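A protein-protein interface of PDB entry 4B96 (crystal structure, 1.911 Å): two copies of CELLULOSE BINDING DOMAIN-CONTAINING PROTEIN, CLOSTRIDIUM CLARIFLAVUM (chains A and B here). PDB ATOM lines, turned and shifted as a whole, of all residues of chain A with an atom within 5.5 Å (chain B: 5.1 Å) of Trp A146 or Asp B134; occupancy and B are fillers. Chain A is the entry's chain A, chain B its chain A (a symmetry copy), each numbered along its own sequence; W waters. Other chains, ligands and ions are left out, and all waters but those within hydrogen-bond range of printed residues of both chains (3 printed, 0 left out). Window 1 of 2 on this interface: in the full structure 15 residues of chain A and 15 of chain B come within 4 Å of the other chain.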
ATOM      1  N   MET A   3      -1.240 -29.265  -1.310  1.00  0.00           N
ATOM      2  CA  MET A   3      -0.682 -28.200  -0.476  1.00  0.00           C
ATOM      3  C   MET A   3       0.621 -27.734  -1.107  1.00  0.00           C
ATOM      4  O   MET A   3       1.380 -28.561  -1.568  1.00  0.00           O
ATOM      5  CB  MET A   3      -0.337 -28.746   0.912  1.00  0.00           C
ATOM      6  CG  MET A   3      -1.466 -29.071   1.769  1.00  0.00           C
ATOM      7  SD  MET A   3      -0.824 -30.032   3.154  1.00  0.00           S
ATOM      8  CE  MET A   3       0.512 -28.937   3.714  1.00  0.00           C
ATOM      9  N   LEU A   5       2.730 -25.320   0.630  1.00  0.00           N
ATOM     10  CA  LEU A   5       3.643 -24.787   1.636  1.00  0.00           C
ATOM     11  C   LEU A   5       3.459 -25.434   2.993  1.00  0.00           C
ATOM     12  O   LEU A   5       2.364 -25.942   3.314  1.00  0.00           O
ATOM     13  CB  LEU A   5       3.550 -23.248   1.749  1.00  0.00           C
ATOM     14  CG  LEU A   5       2.516 -22.446   2.494  1.00  0.00           C
ATOM     15  CD1 LEU A   5       2.581 -22.575   4.070  1.00  0.00           C
ATOM     16  CD2 LEU A   5       2.786 -20.979   2.118  1.00  0.00           C
ATOM     17  N   LYS A   6       4.536 -25.424   3.780  1.00  0.00           N
ATOM     18  CA  LYS A   6       4.474 -25.939   5.176  1.00  0.00           C
ATOM     19  C   LYS A   6       5.264 -24.961   6.020  1.00  0.00           C
ATOM     20  O   LYS A   6       6.096 -24.226   5.494  1.00  0.00           O
ATOM     21  CB  LYS A   6       5.114 -27.325   5.296  1.00  0.00           C
ATOM     22  CG  LYS A   6       4.457 -28.360   4.344  1.00  0.00           C
ATOM     23  CD  LYS A   6       5.019 -29.758   4.660  1.00  0.00           C
ATOM     24  CE  LYS A   6       4.316 -30.839   3.841  1.00  0.00           C
ATOM     25  NZ  LYS A   6       5.035 -32.131   4.027  1.00  0.00           N
ATOM     26  N   LEU A   7       5.012 -24.929   7.327  1.00  0.00           N
ATOM     27  CA  LEU A   7       5.732 -23.992   8.179  1.00  0.00           C
ATOM     28  C   LEU A   7       6.462 -24.763   9.300  1.00  0.00           C
ATOM     29  O   LEU A   7       5.880 -25.677   9.925  1.00  0.00           O
ATOM     30  CB  LEU A   7       4.721 -23.015   8.819  1.00  0.00           C
ATOM     31  CG  LEU A   7       5.356 -22.054   9.838  1.00  0.00           C
ATOM     32  CD1 LEU A   7       4.675 -20.704   9.859  1.00  0.00           C
ATOM     33  CD2 LEU A   7       5.283 -22.611  11.271  1.00  0.00           C
ATOM     34  N   TYR A 132       7.986 -28.798  12.153  1.00  0.00           N
ATOM     35  CA  TYR A 132       6.618 -28.420  11.672  1.00  0.00           C
ATOM     36  C   TYR A 132       5.743 -28.046  12.858  1.00  0.00           C
ATOM     37  O   TYR A 132       5.751 -28.733  13.875  1.00  0.00           O
ATOM     38  CB  TYR A 132       5.967 -29.594  10.933  1.00  0.00           C
ATOM     39  CG  TYR A 132       6.709 -29.846   9.617  1.00  0.00           C
ATOM     40  CD1 TYR A 132       6.790 -28.810   8.654  1.00  0.00           C
ATOM     41  CD2 TYR A 132       7.372 -31.053   9.372  1.00  0.00           C
ATOM     42  CE1 TYR A 132       7.485 -29.011   7.458  1.00  0.00           C
ATOM     43  CE2 TYR A 132       8.075 -31.271   8.152  1.00  0.00           C
ATOM     44  CZ  TYR A 132       8.115 -30.230   7.214  1.00  0.00           C
ATOM     45  OH  TYR A 132       8.843 -30.381   6.033  1.00  0.00           O
ATOM     46  N   TRP A 133       5.017 -26.959  12.756  1.00  0.00           N
ATOM     47  CA  TRP A 133       4.340 -26.505  13.940  1.00  0.00           C
ATOM     48  C   TRP A 133       2.984 -26.021  13.487  1.00  0.00           C
ATOM     49  O   TRP A 133       2.888 -25.015  12.771  1.00  0.00           O
ATOM     50  CB  TRP A 133       5.108 -25.303  14.467  1.00  0.00           C
ATOM     51  CG  TRP A 133       4.554 -24.752  15.788  1.00  0.00           C
ATOM     52  CD1 TRP A 133       4.485 -23.433  16.126  1.00  0.00           C
ATOM     53  CD2 TRP A 133       4.082 -25.500  16.948  1.00  0.00           C
ATOM     54  NE1 TRP A 133       3.998 -23.297  17.417  1.00  0.00           N
ATOM     55  CE2 TRP A 133       3.732 -24.549  17.934  1.00  0.00           C
ATOM     56  CE3 TRP A 133       3.873 -26.873  17.222  1.00  0.00           C
ATOM     57  CZ2 TRP A 133       3.210 -24.921  19.193  1.00  0.00           C
ATOM     58  CZ3 TRP A 133       3.356 -27.256  18.467  1.00  0.00           C
ATOM     59  CH2 TRP A 133       3.012 -26.277  19.440  1.00  0.00           C
ATOM     60  N   ASP A 134       1.932 -26.704  13.916  1.00  0.00           N
ATOM     61  CA  ASP A 134       0.606 -26.330  13.420  1.00  0.00           C
ATOM     62  C   ASP A 134      -0.147 -25.359  14.319  1.00  0.00           C
ATOM     63  O   ASP A 134      -1.371 -25.261  14.172  1.00  0.00           O
ATOM     64  CB  ASP A 134      -0.273 -27.583  13.261  1.00  0.00           C
ATOM     65  CG  ASP A 134      -0.341 -28.420  14.511  1.00  0.00           C
ATOM     66  OD1 ASP A 134      -0.006 -27.927  15.600  1.00  0.00           O
ATOM     67  OD2 ASP A 134      -0.749 -29.591  14.408  1.00  0.00           O
ATOM     68  N   LYS A 135       0.552 -24.674  15.246  1.00  0.00           N
ATOM     69  CA  LYS A 135      -0.090 -23.649  16.094  1.00  0.00           C
ATOM     70  C   LYS A 135       0.339 -22.255  15.703  1.00  0.00           C
ATOM     71  O   LYS A 135      -0.013 -21.266  16.340  1.00  0.00           O
ATOM     72  CB  LYS A 135       0.109 -23.925  17.613  1.00  0.00           C
ATOM     73  CG  LYS A 135      -0.529 -25.297  18.002  1.00  0.00           C
ATOM     74  CD  LYS A 135      -0.415 -25.517  19.509  1.00  0.00           C
ATOM     75  CE  LYS A 135      -1.502 -24.744  20.266  1.00  0.00           C
ATOM     76  NZ  LYS A 135      -1.174 -24.723  21.726  1.00  0.00           N
ATOM     77  N   MET A 136       1.055 -22.143  14.590  1.00  0.00           N
ATOM     78  CA  MET A 136       1.158 -20.848  13.922  1.00  0.00           C
ATOM     79  C   MET A 136       0.429 -20.965  12.597  1.00  0.00           C
ATOM     80  O   MET A 136       0.426 -22.054  12.018  1.00  0.00           O
ATOM     81  CB  MET A 136       2.645 -20.453  13.667  1.00  0.00           C
ATOM     82  CG  MET A 136       3.340 -20.063  14.997  1.00  0.00           C
ATOM     83  SD  MET A 136       5.096 -19.771  14.696  1.00  0.00           S
ATOM     84  CE  MET A 136       5.117 -18.366  13.589  1.00  0.00           C
ATOM     85  N   THR A 137      -0.186 -19.874  12.115  1.00  0.00           N
ATOM     86  CA  THR A 137      -0.951 -19.979  10.862  1.00  0.00           C
ATOM     87  C   THR A 137      -0.328 -19.231   9.672  1.00  0.00           C
ATOM     88  O   THR A 137       0.367 -18.232   9.844  1.00  0.00           O
ATOM     89  CB  THR A 137      -2.376 -19.477  11.040  1.00  0.00           C
ATOM     90  OG1 THR A 137      -2.371 -18.210  11.699  1.00  0.00           O
ATOM     91  CG2 THR A 137      -3.179 -20.502  11.948  1.00  0.00           C
ATOM     92  N   VAL A 138      -0.651 -19.689   8.461  1.00  0.00           N
ATOM     93  CA  VAL A 138      -0.187 -19.008   7.250  1.00  0.00           C
ATOM     94  C   VAL A 138      -1.407 -18.792   6.363  1.00  0.00           C
ATOM     95  O   VAL A 138      -2.268 -19.695   6.233  1.00  0.00           O
ATOM     96  CB  VAL A 138       0.885 -19.864   6.453  1.00  0.00           C
ATOM     97  CG1 VAL A 138       1.437 -19.012   5.300  1.00  0.00           C
ATOM     98  CG2 VAL A 138       2.011 -20.278   7.373  1.00  0.00           C
ATOM     99  N   LEU A 144      -6.673 -19.467   4.679  1.00  0.00           N
ATOM    100  CA  LEU A 144      -5.831 -20.128   5.679  1.00  0.00           C
ATOM    101  C   LEU A 144      -5.225 -21.360   5.009  1.00  0.00           C
ATOM    102  O   LEU A 144      -5.971 -22.210   4.512  1.00  0.00           O
ATOM    103  CB  LEU A 144      -6.708 -20.581   6.872  1.00  0.00           C
ATOM    104  CG  LEU A 144      -5.991 -21.437   7.923  1.00  0.00           C
ATOM    105  CD1 LEU A 144      -4.775 -20.693   8.576  1.00  0.00           C
ATOM    106  CD2 LEU A 144      -7.053 -21.789   9.019  1.00  0.00           C
ATOM    107  N   VAL A 145      -3.897 -21.446   4.909  1.00  0.00           N
ATOM    108  CA  VAL A 145      -3.273 -22.538   4.151  1.00  0.00           C
ATOM    109  C   VAL A 145      -2.411 -23.442   5.028  1.00  0.00           C
ATOM    110  O   VAL A 145      -1.868 -24.429   4.537  1.00  0.00           O
ATOM    111  CB  VAL A 145      -2.444 -22.050   2.934  1.00  0.00           C
ATOM    112  CG1 VAL A 145      -3.337 -21.303   1.965  1.00  0.00           C
ATOM    113  CG2 VAL A 145      -1.241 -21.165   3.427  1.00  0.00           C
ATOM    114  N   TRP A 146      -2.313 -23.118   6.324  1.00  0.00           N
ATOM    115  CA  TRP A 146      -1.469 -23.893   7.218  1.00  0.00           C
ATOM    116  C   TRP A 146      -1.839 -23.511   8.623  1.00  0.00           C
ATOM    117  O   TRP A 146      -1.986 -22.318   8.923  1.00  0.00           O
ATOM    118  CB  TRP A 146       0.044 -23.534   7.033  1.00  0.00           C
ATOM    119  CG  TRP A 146       0.882 -24.242   8.081  1.00  0.00           C
ATOM    120  CD1 TRP A 146       1.227 -23.751   9.368  1.00  0.00           C
ATOM    121  CD2 TRP A 146       1.397 -25.574   8.019  1.00  0.00           C
ATOM    122  NE1 TRP A 146       1.905 -24.733  10.062  1.00  0.00           N
ATOM    123  CE2 TRP A 146       2.033 -25.840   9.261  1.00  0.00           C
ATOM    124  CE3 TRP A 146       1.420 -26.572   7.015  1.00  0.00           C
ATOM    125  CZ2 TRP A 146       2.686 -27.052   9.522  1.00  0.00           C
ATOM    126  CZ3 TRP A 146       2.031 -27.808   7.299  1.00  0.00           C
ATOM    127  CH2 TRP A 146       2.682 -28.025   8.537  1.00  0.00           C
ATOM    128  N   GLY A 147      -1.970 -24.509   9.488  1.00  0.00           N
ATOM    129  CA  GLY A 147      -2.068 -24.235  10.910  1.00  0.00           C
ATOM    130  C   GLY A 147      -3.481 -24.204  11.474  1.00  0.00           C
ATOM    131  O   GLY A 147      -4.462 -24.268  10.724  1.00  0.00           O
ATOM    132  N   ILE A 148      -3.577 -24.087  12.798  1.00  0.00           N
ATOM    133  CA  ILE A 148      -4.865 -24.104  13.508  1.00  0.00           C
ATOM    134  C   ILE A 148      -5.006 -22.823  14.302  1.00  0.00           C
ATOM    135  O   ILE A 148      -4.144 -22.479  15.151  1.00  0.00           O
ATOM    136  CB  ILE A 148      -4.909 -25.324  14.463  1.00  0.00           C
ATOM    137  CG1 ILE A 148      -4.693 -26.630  13.655  1.00  0.00           C
ATOM    138  CG2 ILE A 148      -6.253 -25.372  15.254  1.00  0.00           C
ATOM    139  CD1 ILE A 148      -4.299 -27.843  14.522  1.00  0.00           C
ATOM    140  N   TYR B 132      -0.728 -38.955  11.133  1.00  0.00           N
ATOM    141  CA  TYR B 132      -1.343 -37.590  11.201  1.00  0.00           C
ATOM    142  C   TYR B 132      -1.521 -37.038   9.796  1.00  0.00           C
ATOM    143  O   TYR B 132      -0.622 -37.148   8.967  1.00  0.00           O
ATOM    144  CB  TYR B 132      -0.442 -36.635  11.992  1.00  0.00           C
ATOM    145  CG  TYR B 132      -0.425 -37.051  13.467  1.00  0.00           C
ATOM    146  CD1 TYR B 132      -1.641 -37.089  14.193  1.00  0.00           C
ATOM    147  CD2 TYR B 132       0.754 -37.463  14.095  1.00  0.00           C
ATOM    148  CE1 TYR B 132      -1.651 -37.491  15.531  1.00  0.00           C
ATOM    149  CE2 TYR B 132       0.757 -37.864  15.462  1.00  0.00           C
ATOM    150  CZ  TYR B 132      -0.462 -37.870  16.155  1.00  0.00           C
ATOM    151  OH  TYR B 132      -0.514 -38.314  17.476  1.00  0.00           O
ATOM    152  N   TRP B 133      -2.671 -36.476   9.505  1.00  0.00           N
ATOM    153  CA  TRP B 133      -2.906 -36.127   8.132  1.00  0.00           C
ATOM    154  C   TRP B 133      -3.617 -34.796   8.154  1.00  0.00           C
ATOM    155  O   TRP B 133      -4.764 -34.709   8.610  1.00  0.00           O
ATOM    156  CB  TRP B 133      -3.871 -37.157   7.564  1.00  0.00           C
ATOM    157  CG  TRP B 133      -4.158 -36.970   6.068  1.00  0.00           C
ATOM    158  CD1 TRP B 133      -5.363 -37.168   5.464  1.00  0.00           C
ATOM    159  CD2 TRP B 133      -3.215 -36.635   5.006  1.00  0.00           C
ATOM    160  NE1 TRP B 133      -5.249 -36.978   4.095  1.00  0.00           N
ATOM    161  CE2 TRP B 133      -3.946 -36.638   3.795  1.00  0.00           C
ATOM    162  CE3 TRP B 133      -1.845 -36.283   4.974  1.00  0.00           C
ATOM    163  CZ2 TRP B 133      -3.349 -36.331   2.551  1.00  0.00           C
ATOM    164  CZ3 TRP B 133      -1.240 -35.977   3.747  1.00  0.00           C
ATOM    165  CH2 TRP B 133      -1.999 -35.986   2.544  1.00  0.00           C
ATOM    166  N   ASP B 134      -2.964 -33.763   7.642  1.00  0.00           N
ATOM    167  CA  ASP B 134      -3.574 -32.436   7.735  1.00  0.00           C
ATOM    168  C   ASP B 134      -4.384 -32.032   6.509  1.00  0.00           C
ATOM    169  O   ASP B 134      -4.638 -30.832   6.349  1.00  0.00           O
ATOM    170  CB  ASP B 134      -2.486 -31.364   7.936  1.00  0.00           C
ATOM    171  CG  ASP B 134      -1.397 -31.427   6.900  1.00  0.00           C
ATOM    172  OD1 ASP B 134      -1.591 -32.044   5.840  1.00  0.00           O
ATOM    173  OD2 ASP B 134      -0.328 -30.836   7.140  1.00  0.00           O
ATOM    174  N   LYS B 135      -4.764 -32.998   5.650  1.00  0.00           N
ATOM    175  CA  LYS B 135      -5.626 -32.700   4.487  1.00  0.00           C
ATOM    176  C   LYS B 135      -7.022 -33.245   4.678  1.00  0.00           C
ATOM    177  O   LYS B 135      -7.869 -33.181   3.790  1.00  0.00           O
ATOM    178  CB  LYS B 135      -4.990 -33.159   3.143  1.00  0.00           C
ATOM    179  CG  LYS B 135      -3.638 -32.415   2.903  1.00  0.00           C
ATOM    180  CD  LYS B 135      -3.066 -32.797   1.538  1.00  0.00           C
ATOM    181  CE  LYS B 135      -3.751 -32.012   0.412  1.00  0.00           C
ATOM    182  NZ  LYS B 135      -3.404 -32.628  -0.907  1.00  0.00           N
ATOM    183  N   MET B 136      -7.313 -33.730   5.879  1.00  0.00           N
ATOM    184  CA  MET B 136      -8.709 -33.889   6.277  1.00  0.00           C
ATOM    185  C   MET B 136      -8.975 -32.899   7.395  1.00  0.00           C
ATOM    186  O   MET B 136      -8.054 -32.616   8.165  1.00  0.00           O
ATOM    187  CB  MET B 136      -9.000 -35.336   6.782  1.00  0.00           C
ATOM    188  CG  MET B 136      -9.001 -36.335   5.597  1.00  0.00           C
ATOM    189  SD  MET B 136      -9.175 -38.017   6.226  1.00  0.00           S
ATOM    190  CE  MET B 136     -10.787 -38.024   7.002  1.00  0.00           C
ATOM    191  N   TRP B 146      -8.609 -28.657  13.173  1.00  0.00           N
ATOM    192  CA  TRP B 146      -7.567 -29.538  12.672  1.00  0.00           C
ATOM    193  C   TRP B 146      -7.652 -29.522  11.173  1.00  0.00           C
ATOM    194  O   TRP B 146      -8.754 -29.618  10.612  1.00  0.00           O
ATOM    195  CB  TRP B 146      -7.804 -31.019  13.122  1.00  0.00           C
ATOM    196  CG  TRP B 146      -6.793 -31.936  12.460  1.00  0.00           C
ATOM    197  CD1 TRP B 146      -6.938 -32.604  11.215  1.00  0.00           C
ATOM    198  CD2 TRP B 146      -5.467 -32.224  12.907  1.00  0.00           C
ATOM    199  NE1 TRP B 146      -5.759 -33.254  10.908  1.00  0.00           N
ATOM    200  CE2 TRP B 146      -4.858 -33.051  11.923  1.00  0.00           C
ATOM    201  CE3 TRP B 146      -4.728 -31.895  14.068  1.00  0.00           C
ATOM    202  CZ2 TRP B 146      -3.559 -33.554  12.069  1.00  0.00           C
ATOM    203  CZ3 TRP B 146      -3.404 -32.358  14.187  1.00  0.00           C
ATOM    204  CH2 TRP B 146      -2.844 -33.206  13.202  1.00  0.00           C
ATOM    205  N   GLY B 147      -6.501 -29.420  10.519  1.00  0.00           N
ATOM    206  CA  GLY B 147      -6.449 -29.653   9.088  1.00  0.00           C
ATOM    207  C   GLY B 147      -6.493 -28.403   8.220  1.00  0.00           C
ATOM    208  O   GLY B 147      -6.703 -27.293   8.722  1.00  0.00           O
ATOM    209  N   ILE B 148      -6.313 -28.595   6.914  1.00  0.00           N
ATOM    210  CA  ILE B 148      -6.264 -27.490   5.946  1.00  0.00           C
ATOM    211  C   ILE B 148      -7.336 -27.704   4.899  1.00  0.00           C
ATOM    212  O   ILE B 148      -7.386 -28.761   4.219  1.00  0.00           O
ATOM    213  CB  ILE B 148      -4.869 -27.457   5.273  1.00  0.00           C
ATOM    214  CG1 ILE B 148      -3.767 -27.308   6.355  1.00  0.00           C
ATOM    215  CG2 ILE B 148      -4.777 -26.308   4.221  1.00  0.00           C
ATOM    216  CD1 ILE B 148      -2.354 -27.683   5.864  1.00  0.00           C
HETATM  217  O   HOH W   1      -5.608 -24.849   8.095  1.00  0.00           O
HETATM  218  O   HOH W   2       0.752 -32.921   4.412  1.00  0.00           O
HETATM  219  O   HOH W   3      -6.861 -25.567  11.080  1.00  0.00           O
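The side-chain sulfur (SD) of Met A3 lies close to the side-chain carboxylate (OD1) of Asp B134.
The backbone carbonyl oxygen (O) of Trp A133 is in hydrogen-bond range of the indole nitrogen (NE1) of Trp A146 (2.9 Å).
The backbone carbonyl oxygen (O) of Asp A134 sits at hydrogen-bond distance from the backbone NH (N) of Ile A148 (2.9 Å).
The backbone carbonyl oxygen (O) of Val A138 lies within hydrogen-bond range of the backbone NH (N) of Val A145 (2.7 Å).
N of Val A138 sits at hydrogen-bond distance from O of Trp A146, 3.0 Å away.
O of Trp B133 lies within hydrogen-bond range of NE1 of Trp B146.
O of Asp B134 sits at hydrogen-bond distance from N of Ile B148, 2.9 Å away.
Among the printed residues, merely in contact across the chains: Val A145 with Ile B148 (3.5 Å), Met A3 with Lys B135 (3.7 Å), Met A3 with Ile B148 (3.8 Å), Asp A134 with Trp B146 (3.8 Å) and Trp A146 with Asp B134 (3.8 Å).
Of the printed residues of chain B, Met A3 touches Asp B134, Lys B135 and Ile B148.
Printed residues of chain B within 4 Å of Asp A134: Trp B146.
Of the printed residues of chain B, Trp A146 touches Asp B134.
Of the printed residues of chain A, Asp B134 touches Met A3 (3.4 Å) and Trp A146 (3.8 Å).
Of the printed residues of chain A, Lys B135 touches Met A3 (3.7 Å).
Of the printed residues of chain A, Ile B148 touches Met A3 and Val A145.
The nearest printed residue of chain B that does not touch Trp A146 is Ile B148 (4.1 Å).
The nearest printed residue of chain A that does not touch Asp B134 is Lys A6 (5.7 Å).
Hydrophobic or aromatic side chains of chain B that line the printed part of chain A: Trp B146 and Ile B148.
Along chain A the printed residues that touch a printed residue of chain B span positions 3 to 146.
Among the printed residues, 6 pairs touch across the chains.
Asp A134 touches Trp B146, and with the chains exchanged Trp A146 touches Asp B134.
Of the 6 pairs that touch across the chains among the printed residues, 2 have their exchanged pair printed and touching as well.
Water W3 bridges the backbone carbonyl oxygen of Gly A147 and the backbone carbonyl oxygen of Gly B147.
Water W1 lies within hydrogen-bond range of the backbone carbonyl oxygen (O) of Gly B147 (2.8 Å) and the backbone carbonyl oxygen (O) of Gly A147 (2.9 Å).
Water W2 lies within hydrogen-bond range of OD1 of Asp B134 and SD of Met A3.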
